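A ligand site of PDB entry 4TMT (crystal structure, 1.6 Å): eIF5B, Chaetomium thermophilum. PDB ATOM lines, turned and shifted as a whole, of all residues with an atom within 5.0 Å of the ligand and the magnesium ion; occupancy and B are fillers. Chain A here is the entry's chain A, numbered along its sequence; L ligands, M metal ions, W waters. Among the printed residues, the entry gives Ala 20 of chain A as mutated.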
ATOM      1  N   GLY A  17       5.691 -24.086   8.578  1.00  0.00           N
ATOM      2  CA  GLY A  17       5.124 -23.448   9.750  1.00  0.00           C
ATOM      3  C   GLY A  17       3.870 -24.153  10.209  1.00  0.00           C
ATOM      4  O   GLY A  17       3.317 -25.013   9.514  1.00  0.00           O
ATOM      5  N   HIS A  18       3.404 -23.769  11.399  1.00  0.00           N
ATOM      6  CA  HIS A  18       2.244 -24.375  12.033  1.00  0.00           C
ATOM      7  C   HIS A  18       1.003 -24.080  11.227  1.00  0.00           C
ATOM      8  O   HIS A  18       0.986 -23.168  10.383  1.00  0.00           O
ATOM      9  CB  HIS A  18       2.140 -23.823  13.471  1.00  0.00           C
ATOM     10  CG  HIS A  18       1.180 -24.542  14.363  1.00  0.00           C
ATOM     11  ND1 HIS A  18       1.470 -25.747  14.973  1.00  0.00           N
ATOM     12  CD2 HIS A  18      -0.063 -24.199  14.784  1.00  0.00           C
ATOM     13  CE1 HIS A  18       0.448 -26.116  15.717  1.00  0.00           C
ATOM     14  NE2 HIS A  18      -0.492 -25.197  15.628  1.00  0.00           N
ATOM     15  N   VAL A  19      -0.054 -24.844  11.491  1.00  0.00           N
ATOM     16  CA  VAL A  19      -1.348 -24.600  10.857  1.00  0.00           C
ATOM     17  C   VAL A  19      -1.786 -23.128  11.016  1.00  0.00           C
ATOM     18  O   VAL A  19      -1.506 -22.498  12.054  1.00  0.00           O
ATOM     19  CB  VAL A  19      -2.475 -25.464  11.438  1.00  0.00           C
ATOM     20  CG1 VAL A  19      -2.291 -26.888  11.019  1.00  0.00           C
ATOM     21  CG2 VAL A  19      -2.540 -25.345  12.979  1.00  0.00           C
ATOM     22  N   ALA A  20      -2.387 -22.604   9.952  1.00  0.00           N
ATOM     23  CA  ALA A  20      -3.084 -21.314   9.965  1.00  0.00           C
ATOM     24  C   ALA A  20      -2.156 -20.128  10.221  1.00  0.00           C
ATOM     25  O   ALA A  20      -2.647 -19.030  10.543  1.00  0.00           O
ATOM     26  CB  ALA A  20      -4.232 -21.341  11.006  1.00  0.00           C
ATOM     27  N   THR A  21      -0.854 -20.291   9.999  1.00  0.00           N
ATOM     28  CA  THR A  21       0.046 -19.156  10.271  1.00  0.00           C
ATOM     29  C   THR A  21       0.095 -18.192   9.102  1.00  0.00           C
ATOM     30  O   THR A  21       0.543 -17.067   9.275  1.00  0.00           O
ATOM     31  CB  THR A  21       1.468 -19.620  10.598  1.00  0.00           C
ATOM     32  OG1 THR A  21       1.901 -20.577   9.607  1.00  0.00           O
ATOM     33  CG2 THR A  21       1.488 -20.288  12.006  1.00  0.00           C
ATOM     34  N   GLY A  22      -0.403 -18.623   7.931  1.00  0.00           N
ATOM     35  CA  GLY A  22      -0.472 -17.771   6.755  1.00  0.00           C
ATOM     36  C   GLY A  22       0.480 -18.087   5.596  1.00  0.00           C
ATOM     37  O   GLY A  22       0.749 -17.190   4.769  1.00  0.00           O
ATOM     38  N   LYS A  23       1.009 -19.299   5.558  1.00  0.00           N
ATOM     39  CA  LYS A  23       1.902 -19.710   4.460  1.00  0.00           C
ATOM     40  C   LYS A  23       1.264 -19.553   3.078  1.00  0.00           C
ATOM     41  O   LYS A  23       1.813 -18.870   2.175  1.00  0.00           O
ATOM     42  CB  LYS A  23       2.305 -21.187   4.647  1.00  0.00           C
ATOM     43  CG  LYS A  23       3.023 -21.457   5.994  1.00  0.00           C
ATOM     44  CD  LYS A  23       3.453 -22.942   6.149  1.00  0.00           C
ATOM     45  CE  LYS A  23       2.238 -23.860   6.299  1.00  0.00           C
ATOM     46  NZ  LYS A  23       1.422 -23.660   7.555  1.00  0.00           N
ATOM     47  N   THR A  24       0.091 -20.156   2.916  1.00  0.00           N
ATOM     48  CA  THR A  24      -0.606 -20.090   1.641  1.00  0.00           C
ATOM     49  C   THR A  24      -1.082 -18.665   1.363  1.00  0.00           C
ATOM     50  O   THR A  24      -0.965 -18.158   0.232  1.00  0.00           O
ATOM     51  CB  THR A  24      -1.781 -21.057   1.614  1.00  0.00           C
ATOM     52  OG1 THR A  24      -1.287 -22.378   1.934  1.00  0.00           O
ATOM     53  CG2 THR A  24      -2.473 -21.076   0.219  1.00  0.00           C
ATOM     54  N   LYS A  25      -1.566 -17.976   2.415  1.00  0.00           N
ATOM     55  CA  LYS A  25      -2.021 -16.594   2.213  1.00  0.00           C
ATOM     56  C   LYS A  25      -0.884 -15.677   1.757  1.00  0.00           C
ATOM     57  O   LYS A  25      -1.118 -14.787   0.907  1.00  0.00           O
ATOM     58  CB  LYS A  25      -2.654 -16.071   3.520  1.00  0.00           C
ATOM     59  CG  LYS A  25      -3.704 -14.986   3.320  1.00  0.00           C
ATOM     60  CD  LYS A  25      -5.009 -15.615   2.775  1.00  0.00           C
ATOM     61  CE  LYS A  25      -6.130 -14.618   2.596  1.00  0.00           C
ATOM     62  NZ  LYS A  25      -7.264 -15.323   1.921  1.00  0.00           N
ATOM     63  N   GLN A  36      -6.078 -20.056  -1.150  1.00  0.00           N
ATOM     64  CA  GLN A  36      -6.518 -20.336   0.205  1.00  0.00           C
ATOM     65  C   GLN A  36      -8.054 -20.371   0.314  1.00  0.00           C
ATOM     66  O   GLN A  36      -8.602 -21.205   0.997  1.00  0.00           O
ATOM     67  CB  GLN A  36      -5.928 -19.329   1.198  1.00  0.00           C
ATOM     68  CG  GLN A  36      -5.941 -19.797   2.641  1.00  0.00           C
ATOM     69  CD  GLN A  36      -7.231 -19.454   3.368  1.00  0.00           C
ATOM     70  OE1 GLN A  36      -7.941 -18.540   2.970  1.00  0.00           O
ATOM     71  NE2 GLN A  36      -7.546 -20.206   4.413  1.00  0.00           N
ATOM     72  N   GLU A  39      -9.468 -23.730  -0.914  1.00  0.00           N
ATOM     73  CA  GLU A  39      -9.128 -24.955  -0.188  1.00  0.00           C
ATOM     74  C   GLU A  39     -10.223 -25.461   0.697  1.00  0.00           C
ATOM     75  O   GLU A  39     -10.853 -24.683   1.426  1.00  0.00           O
ATOM     76  CB  GLU A  39      -7.872 -24.775   0.684  1.00  0.00           C
ATOM     77  CG  GLU A  39      -6.580 -24.615  -0.093  1.00  0.00           C
ATOM     78  CD  GLU A  39      -5.404 -24.260   0.810  1.00  0.00           C
ATOM     79  OE1 GLU A  39      -5.648 -23.619   1.849  1.00  0.00           O
ATOM     80  OE2 GLU A  39      -4.249 -24.610   0.489  1.00  0.00           O
ATOM     81  N   GLY A  42     -10.118 -24.473   4.223  1.00  0.00           N
ATOM     82  CA  GLY A  42      -9.121 -23.437   4.218  1.00  0.00           C
ATOM     83  C   GLY A  42      -7.729 -23.940   4.548  1.00  0.00           C
ATOM     84  O   GLY A  42      -6.892 -23.151   4.944  1.00  0.00           O
ATOM     85  N   ILE A  43      -7.504 -25.251   4.449  1.00  0.00           N
ATOM     86  CA  ILE A  43      -6.208 -25.821   4.811  1.00  0.00           C
ATOM     87  C   ILE A  43      -5.510 -26.445   3.609  1.00  0.00           C
ATOM     88  O   ILE A  43      -6.149 -26.938   2.664  1.00  0.00           O
ATOM     89  CB  ILE A  43      -6.324 -26.847   5.960  1.00  0.00           C
ATOM     90  CG1 ILE A  43      -6.947 -28.148   5.481  1.00  0.00           C
ATOM     91  CG2 ILE A  43      -7.110 -26.255   7.146  1.00  0.00           C
ATOM     92  CD1 ILE A  43      -6.934 -29.258   6.577  1.00  0.00           C
ATOM     93  N   THR A  44      -4.182 -26.445   3.646  1.00  0.00           N
ATOM     94  CA  THR A  44      -3.376 -27.080   2.604  1.00  0.00           C
ATOM     95  C   THR A  44      -3.187 -28.571   2.867  1.00  0.00           C
ATOM     96  O   THR A  44      -2.904 -28.950   4.012  1.00  0.00           O
ATOM     97  CB  THR A  44      -2.041 -26.382   2.509  1.00  0.00           C
ATOM     98  OG1 THR A  44      -2.296 -24.985   2.235  1.00  0.00           O
ATOM     99  CG2 THR A  44      -1.160 -26.993   1.396  1.00  0.00           C
ATOM    100  N   ASP A  81       4.952 -24.760  -1.193  1.00  0.00           N
ATOM    101  CA  ASP A  81       4.016 -24.583  -0.062  1.00  0.00           C
ATOM    102  C   ASP A  81       3.810 -25.957   0.592  1.00  0.00           C
ATOM    103  O   ASP A  81       3.787 -26.972  -0.093  1.00  0.00           O
ATOM    104  CB  ASP A  81       2.703 -23.947  -0.588  1.00  0.00           C
ATOM    105  CG  ASP A  81       1.723 -23.499   0.512  1.00  0.00           C
ATOM    106  OD1 ASP A  81       2.081 -23.558   1.718  1.00  0.00           O
ATOM    107  OD2 ASP A  81       0.576 -23.134   0.153  1.00  0.00           O
ATOM    108  N   THR A  82       3.713 -25.998   1.930  1.00  0.00           N
ATOM    109  CA  THR A  82       3.510 -27.278   2.629  1.00  0.00           C
ATOM    110  C   THR A  82       2.340 -27.213   3.610  1.00  0.00           C
ATOM    111  O   THR A  82       2.035 -26.146   4.110  1.00  0.00           O
ATOM    112  CB  THR A  82       4.770 -27.717   3.442  1.00  0.00           C
ATOM    113  OG1 THR A  82       5.040 -26.728   4.453  1.00  0.00           O
ATOM    114  CG2 THR A  82       5.960 -27.862   2.510  1.00  0.00           C
ATOM    115  N   PRO A  83       1.706 -28.345   3.872  1.00  0.00           N
ATOM    116  CA  PRO A  83       0.669 -28.381   4.916  1.00  0.00           C
ATOM    117  C   PRO A  83       1.269 -28.188   6.278  1.00  0.00           C
ATOM    118  O   PRO A  83       2.301 -28.800   6.585  1.00  0.00           O
ATOM    119  CB  PRO A  83       0.081 -29.801   4.832  1.00  0.00           C
ATOM    120  CG  PRO A  83       0.527 -30.324   3.491  1.00  0.00           C
ATOM    121  CD  PRO A  83       1.856 -29.637   3.186  1.00  0.00           C
ATOM    122  N   GLY A  84       0.608 -27.425   7.126  1.00  0.00           N
ATOM    123  CA  GLY A  84       1.021 -27.363   8.523  1.00  0.00           C
ATOM    124  C   GLY A  84       0.332 -28.386   9.395  1.00  0.00           C
ATOM    125  O   GLY A  84       0.757 -28.632  10.527  1.00  0.00           O
ATOM    126  N   HIS A  85      -0.741 -29.011   8.909  1.00  0.00           N
ATOM    127  CA  HIS A  85      -1.513 -29.912   9.759  1.00  0.00           C
ATOM    128  C   HIS A  85      -0.727 -31.132  10.203  1.00  0.00           C
ATOM    129  O   HIS A  85       0.048 -31.693   9.437  1.00  0.00           O
ATOM    130  CB  HIS A  85      -2.797 -30.335   9.041  1.00  0.00           C
ATOM    131  CG  HIS A  85      -3.779 -31.050   9.910  1.00  0.00           C
ATOM    132  ND1 HIS A  85      -3.673 -32.390  10.223  1.00  0.00           N
ATOM    133  CD2 HIS A  85      -4.915 -30.621  10.523  1.00  0.00           C
ATOM    134  CE1 HIS A  85      -4.686 -32.753  10.996  1.00  0.00           C
ATOM    135  NE2 HIS A  85      -5.445 -31.687  11.191  1.00  0.00           N
ATOM    136  N   ASN A 135       4.350 -13.228  10.847  1.00  0.00           N
ATOM    137  CA  ASN A 135       3.192 -12.851  10.060  1.00  0.00           C
ATOM    138  C   ASN A 135       2.028 -12.370  10.892  1.00  0.00           C
ATOM    139  O   ASN A 135       1.960 -12.578  12.103  1.00  0.00           O
ATOM    140  CB  ASN A 135       2.807 -14.053   9.183  1.00  0.00           C
ATOM    141  CG  ASN A 135       1.795 -13.675   8.099  1.00  0.00           C
ATOM    142  OD1 ASN A 135       1.919 -12.628   7.436  1.00  0.00           O
ATOM    143  ND2 ASN A 135       0.796 -14.510   7.906  1.00  0.00           N
ATOM    144  N   LYS A 136       1.109 -11.674  10.221  1.00  0.00           N
ATOM    145  CA  LYS A 136      -0.144 -11.147  10.780  1.00  0.00           C
ATOM    146  C   LYS A 136       0.072  -9.877  11.630  1.00  0.00           C
ATOM    147  O   LYS A 136      -0.684  -9.595  12.561  1.00  0.00           O
ATOM    148  CB  LYS A 136      -0.902 -12.207  11.600  1.00  0.00           C
ATOM    149  CG  LYS A 136      -1.049 -13.590  10.868  1.00  0.00           C
ATOM    150  CD  LYS A 136      -2.243 -14.346  11.435  1.00  0.00           C
ATOM    151  CE  LYS A 136      -2.314 -15.706  10.781  1.00  0.00           C
ATOM    152  NZ  LYS A 136      -3.470 -16.496  11.353  1.00  0.00           N
ATOM    153  N   ILE A 137       1.046  -9.068  11.235  1.00  0.00           N
ATOM    154  CA  ILE A 137       1.243  -7.797  11.948  1.00  0.00           C
ATOM    155  C   ILE A 137       0.063  -6.841  11.870  1.00  0.00           C
ATOM    156  O   ILE A 137      -0.067  -5.956  12.698  1.00  0.00           O
ATOM    157  CB  ILE A 137       2.500  -7.066  11.448  1.00  0.00           C
ATOM    158  CG1 ILE A 137       2.390  -6.695   9.973  1.00  0.00           C
ATOM    159  CG2 ILE A 137       3.742  -7.919  11.764  1.00  0.00           C
ATOM    160  CD1 ILE A 137       3.669  -5.979   9.426  1.00  0.00           C
ATOM    161  N   ASP A 138      -0.829  -7.037  10.908  1.00  0.00           N
ATOM    162  CA  ASP A 138      -1.991  -6.184  10.829  1.00  0.00           C
ATOM    163  C   ASP A 138      -2.941  -6.436  11.990  1.00  0.00           C
ATOM    164  O   ASP A 138      -3.878  -5.664  12.219  1.00  0.00           O
ATOM    165  CB  ASP A 138      -2.711  -6.404   9.512  1.00  0.00           C
ATOM    166  CG  ASP A 138      -3.177  -7.846   9.367  1.00  0.00           C
ATOM    167  OD1 ASP A 138      -4.395  -8.079   9.550  1.00  0.00           O
ATOM    168  OD2 ASP A 138      -2.319  -8.718   9.107  1.00  0.00           O
ATOM    169  N   ARG A 139      -2.726  -7.548  12.704  1.00  0.00           N
ATOM    170  CA  ARG A 139      -3.552  -7.830  13.861  1.00  0.00           C
ATOM    171  C   ARG A 139      -3.085  -7.103  15.113  1.00  0.00           C
ATOM    172  O   ARG A 139      -3.772  -7.151  16.117  1.00  0.00           O
ATOM    173  CB  ARG A 139      -3.603  -9.335  14.141  1.00  0.00           C
ATOM    174  CG  ARG A 139      -4.216 -10.113  12.976  1.00  0.00           C
ATOM    175  CD  ARG A 139      -4.702 -11.480  13.387  1.00  0.00           C
ATOM    176  NE  ARG A 139      -5.836 -11.370  14.312  1.00  0.00           N
ATOM    177  CZ  ARG A 139      -5.824 -11.852  15.551  1.00  0.00           C
ATOM    178  NH1 ARG A 139      -4.750 -12.470  16.016  1.00  0.00           N
ATOM    179  NH2 ARG A 139      -6.889 -11.706  16.334  1.00  0.00           N
ATOM    180  N   THR A 202       5.590  -9.490   8.671  1.00  0.00           N
ATOM    181  CA  THR A 202       4.801  -9.484   7.443  1.00  0.00           C
ATOM    182  C   THR A 202       3.308  -9.447   7.731  1.00  0.00           C
ATOM    183  O   THR A 202       2.829  -9.829   8.826  1.00  0.00           O
ATOM    184  CB  THR A 202       5.063 -10.747   6.556  1.00  0.00           C
ATOM    185  OG1 THR A 202       4.705 -11.935   7.272  1.00  0.00           O
ATOM    186  CG2 THR A 202       6.558 -10.863   6.113  1.00  0.00           C
ATOM    187  N   SER A 203       2.564  -9.010   6.718  1.00  0.00           N
ATOM    188  CA  SER A 203       1.124  -9.282   6.662  1.00  0.00           C
ATOM    189  C   SER A 203       0.751  -9.826   5.285  1.00  0.00           C
ATOM    190  O   SER A 203       0.932  -9.169   4.272  1.00  0.00           O
ATOM    191  CB  SER A 203       0.283  -8.031   6.957  1.00  0.00           C
ATOM    192  OG  SER A 203      -1.100  -8.320   6.702  1.00  0.00           O
ATOM    193  N   ALA A 204       0.221 -11.027   5.266  1.00  0.00           N
ATOM    194  CA  ALA A 204      -0.343 -11.567   4.037  1.00  0.00           C
ATOM    195  C   ALA A 204      -1.595 -10.817   3.601  1.00  0.00           C
ATOM    196  O   ALA A 204      -1.953 -10.854   2.432  1.00  0.00           O
ATOM    197  CB  ALA A 204      -0.661 -13.067   4.218  1.00  0.00           C
ATOM    198  N   HIS A 205      -2.287 -10.186   4.533  1.00  0.00           N
ATOM    199  CA  HIS A 205      -3.487  -9.440   4.172  1.00  0.00           C
ATOM    200  C   HIS A 205      -3.188  -8.069   3.556  1.00  0.00           C
ATOM    201  O   HIS A 205      -3.869  -7.667   2.608  1.00  0.00           O
ATOM    202  CB  HIS A 205      -4.404  -9.330   5.398  1.00  0.00           C
ATOM    203  CG  HIS A 205      -5.199 -10.569   5.653  1.00  0.00           C
ATOM    204  ND1 HIS A 205      -6.340 -10.578   6.426  1.00  0.00           N
ATOM    205  CD2 HIS A 205      -5.034 -11.836   5.206  1.00  0.00           C
ATOM    206  CE1 HIS A 205      -6.850 -11.798   6.450  1.00  0.00           C
ATOM    207  NE2 HIS A 205      -6.082 -12.585   5.716  1.00  0.00           N
ATOM    208  N   ARG A 293      -0.295 -27.434  -7.776  1.00  0.00           N
ATOM    209  CA  ARG A 293      -1.317 -28.266  -7.124  1.00  0.00           C
ATOM    210  C   ARG A 293      -2.715 -27.870  -7.560  1.00  0.00           C
ATOM    211  O   ARG A 293      -3.721 -28.449  -7.124  1.00  0.00           O
ATOM    212  CB  ARG A 293      -1.166 -28.234  -5.587  1.00  0.00           C
ATOM    213  CG  ARG A 293      -1.474 -26.942  -4.884  1.00  0.00           C
ATOM    214  CD  ARG A 293      -1.255 -27.184  -3.383  1.00  0.00           C
ATOM    215  NE  ARG A 293      -1.070 -25.983  -2.603  1.00  0.00           N
ATOM    216  CZ  ARG A 293      -1.996 -25.457  -1.797  1.00  0.00           C
ATOM    217  NH1 ARG A 293      -3.190 -26.018  -1.669  1.00  0.00           N
ATOM    218  NH2 ARG A 293      -1.723 -24.361  -1.106  1.00  0.00           N
HETATM  219  P1  LIG L   1      -2.097 -24.557   6.648  1.00  0.00           P
HETATM  220  O1  LIG L   1      -2.234 -22.983   6.981  1.00  0.00           O
HETATM  221  S1  LIG L   1      -3.556 -25.365   7.659  1.00  0.00           S
HETATM  222  O2  LIG L   1      -0.701 -25.125   7.145  1.00  0.00           O
HETATM  223  O3  LIG L   1      -2.280 -24.815   5.083  1.00  0.00           O
HETATM  224  P2  LIG L   1      -1.460 -21.733   6.315  1.00  0.00           P
HETATM  225  O4  LIG L   1      -1.369 -21.915   4.838  1.00  0.00           O
HETATM  226  O5  LIG L   1      -0.214 -21.488   7.098  1.00  0.00           O
HETATM  227  P3  LIG L   1      -3.530 -19.867   5.683  1.00  0.00           P
HETATM  228  O6  LIG L   1      -4.556 -20.896   5.377  1.00  0.00           O
HETATM  229  O7  LIG L   1      -2.849 -19.163   4.558  1.00  0.00           O
HETATM  230  O8  LIG L   1      -2.440 -20.520   6.668  1.00  0.00           O
HETATM  231  O9  LIG L   1      -4.186 -18.753   6.625  1.00  0.00           O
HETATM  232  C1  LIG L   1      -4.954 -19.156   7.744  1.00  0.00           C
HETATM  233  C2  LIG L   1      -5.940 -18.056   8.117  1.00  0.00           C
HETATM  234  O10 LIG L   1      -5.203 -16.939   8.606  1.00  0.00           O
HETATM  235  C3  LIG L   1      -6.729 -17.560   6.926  1.00  0.00           C
HETATM  236  O11 LIG L   1      -8.033 -17.197   7.384  1.00  0.00           O
HETATM  237  C4  LIG L   1      -6.009 -16.309   6.493  1.00  0.00           C
HETATM  238  O12 LIG L   1      -6.881 -15.361   5.873  1.00  0.00           O
HETATM  239  C5  LIG L   1      -5.489 -15.790   7.822  1.00  0.00           C
HETATM  240  N1  LIG L   1      -4.270 -14.999   7.627  1.00  0.00           N
HETATM  241  C6  LIG L   1      -3.135 -15.389   7.029  1.00  0.00           C
HETATM  242  N2  LIG L   1      -2.218 -14.398   7.032  1.00  0.00           N
HETATM  243  C7  LIG L   1      -2.774 -13.349   7.657  1.00  0.00           C
HETATM  244  C8  LIG L   1      -2.358 -11.983   8.007  1.00  0.00           C
HETATM  245  O13 LIG L   1      -1.237 -11.584   7.708  1.00  0.00           O
HETATM  246  N3  LIG L   1      -3.244 -11.224   8.652  1.00  0.00           N
HETATM  247  C9  LIG L   1      -4.471 -11.641   8.994  1.00  0.00           C
HETATM  248  N4  LIG L   1      -5.283 -10.799   9.653  1.00  0.00           N
HETATM  249  N5  LIG L   1      -4.914 -12.883   8.710  1.00  0.00           N
HETATM  250  C10 LIG L   1      -4.127 -13.753   8.046  1.00  0.00           C
HETATM  251 MG    MG M   1      -1.842 -23.462   3.593  1.00  0.00          MG
HETATM  252  O   HOH W   1      -2.417 -28.195   6.683  1.00  0.00           O
HETATM  253  O   HOH W   2      -5.346 -22.606   7.645  1.00  0.00           O
HETATM  254  O   HOH W   3       0.243 -24.121   3.496  1.00  0.00           O
HETATM  255  O   HOH W   4      -3.821 -22.701   3.415  1.00  0.00           O
HETATM  256  O   HOH W   5      -9.401 -14.283   7.112  1.00  0.00           O
HETATM  257  O   HOH W   6      -8.088 -16.168  10.359  1.00  0.00           O
HETATM  258  O   HOH W   7      -5.850 -14.613  11.205  1.00  0.00           O
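The magnesium ion is bound by an oxygen (O4) of the ligand (2.0 Å), the side-chain hydroxyl of Thr 24 (2.1 Å), an oxygen (O3) of the ligand (2.1 Å), the side-chain hydroxyl of Thr 44 (2.1 Å), water W4 (2.1 Å) and water W3 (2.2 Å).
O of Gly 42 lies close to O6 of the ligand (3.3 Å). Residues that only touch the ligand: Arg 139, Ile 43, Pro 83, Val 19 and His 18. Hydrophobic or aromatic side chains within 4 Å of the ligand: Val 19, Ala 20, Ile 43, Ala 204 and His 205.
The backbone carbonyl oxygen (O) of Thr 21 lies within hydrogen-bond range of the side-chain amide nitrogen (ND2) of Asn 135 (2.9 Å). OE1 of Gln 36 sits at hydrogen-bond distance from NZ of Lys 25, 3.5 Å away. The backbone NH of His 205 lies within hydrogen-bond range of the side-chain hydroxyl of Ser 203 (3.1 Å). NZ of Lys 136 sits at hydrogen-bond distance from O of Ala 20 (2.8 Å). The side-chain amino group (NZ) of Lys 23 sits at hydrogen-bond distance from the backbone carbonyl oxygen (O) of His 18, at 2.9 Å. The side-chain amide nitrogen (NE2) of Gln 36 lies within hydrogen-bond range of the backbone carbonyl oxygen (O) of Gly 42 (3.1 Å). The backbone carbonyl oxygen (O) of Gly 17 lies within hydrogen-bond range of the side-chain amino group (NZ) of Lys 23, at 3.0 Å. The side-chain carboxylate (OE2) of Glu 39 sits close to the side-chain hydroxyl (OG1) of Thr 44, at 2.6 Å.
An oxygen (O4) of the ligand sits close to the backbone NH of Thr 24 (3.0 Å). N3 of the ligand is in hydrogen-bond range of OD2 of Asp 138. An oxygen (O5) of the ligand is in hydrogen-bond range of the side-chain hydroxyl (OG1) of Thr 21. O2 of the ligand sits at hydrogen-bond distance from N of Gly 84 (2.6 Å). The side-chain amide nitrogen of Asn 135 is in hydrogen-bond range of a nitrogen (N2) of the ligand, at 3.1 Å. O5 of the ligand is in salt-bridge range of NZ of Lys 23, 2.8 Å away. The backbone NH of Thr 21 lies within hydrogen-bond range of an oxygen (O5) of the ligand (3.2 Å). The backbone NH of Lys 136 lies close to an oxygen (O13) of the ligand, 3.4 Å away. N of Thr 44 sits close to O3 of the ligand. A ring nitrogen (NE2) of His 205 is in hydrogen-bond range of an oxygen (O12) of the ligand, at 2.9 Å. The backbone NH (N) of Gly 22 lies within hydrogen-bond range of an oxygen (O5) of the ligand (3.0 Å). N of Lys 25 is in hydrogen-bond range of O7 of the ligand. An oxygen (O6) of the ligand lies within hydrogen-bond range of the side-chain amide nitrogen (NE2) of Gln 36, 3.2 Å away. The backbone NH of Ala 20 is in hydrogen-bond range of an oxygen (O1) of the ligand (3.0 Å). An oxygen (O5) of the ligand sits at hydrogen-bond distance from the backbone NH (N) of Lys 23 (2.9 Å). An oxygen (O10) of the ligand lies within hydrogen-bond range of the side-chain amino group of Lys 136. OG of Ser 203 is in hydrogen-bond range of O13 of the ligand, 3.4 Å away. O13 of the ligand lies within hydrogen-bond range of N of Ala 204 (2.9 Å).
Water W3 lies within hydrogen-bond range of OD1 of Asp 81 and O of Thr 82. Water W4 lies within hydrogen-bond range of OE1 of Glu 39, O6 of the ligand and O of Gly 42. Water W2 bridges an oxygen (O6) of the ligand and the backbone carbonyl oxygen (O) of Gly 42. Water W7 lies within hydrogen-bond range of NZ of Lys 136 (3.0 Å) and N5 of the ligand (3.2 Å). Water W1 lies within hydrogen-bond range of O of Thr 44, N of His 85, N of Gly 84 and S1 of the ligand.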
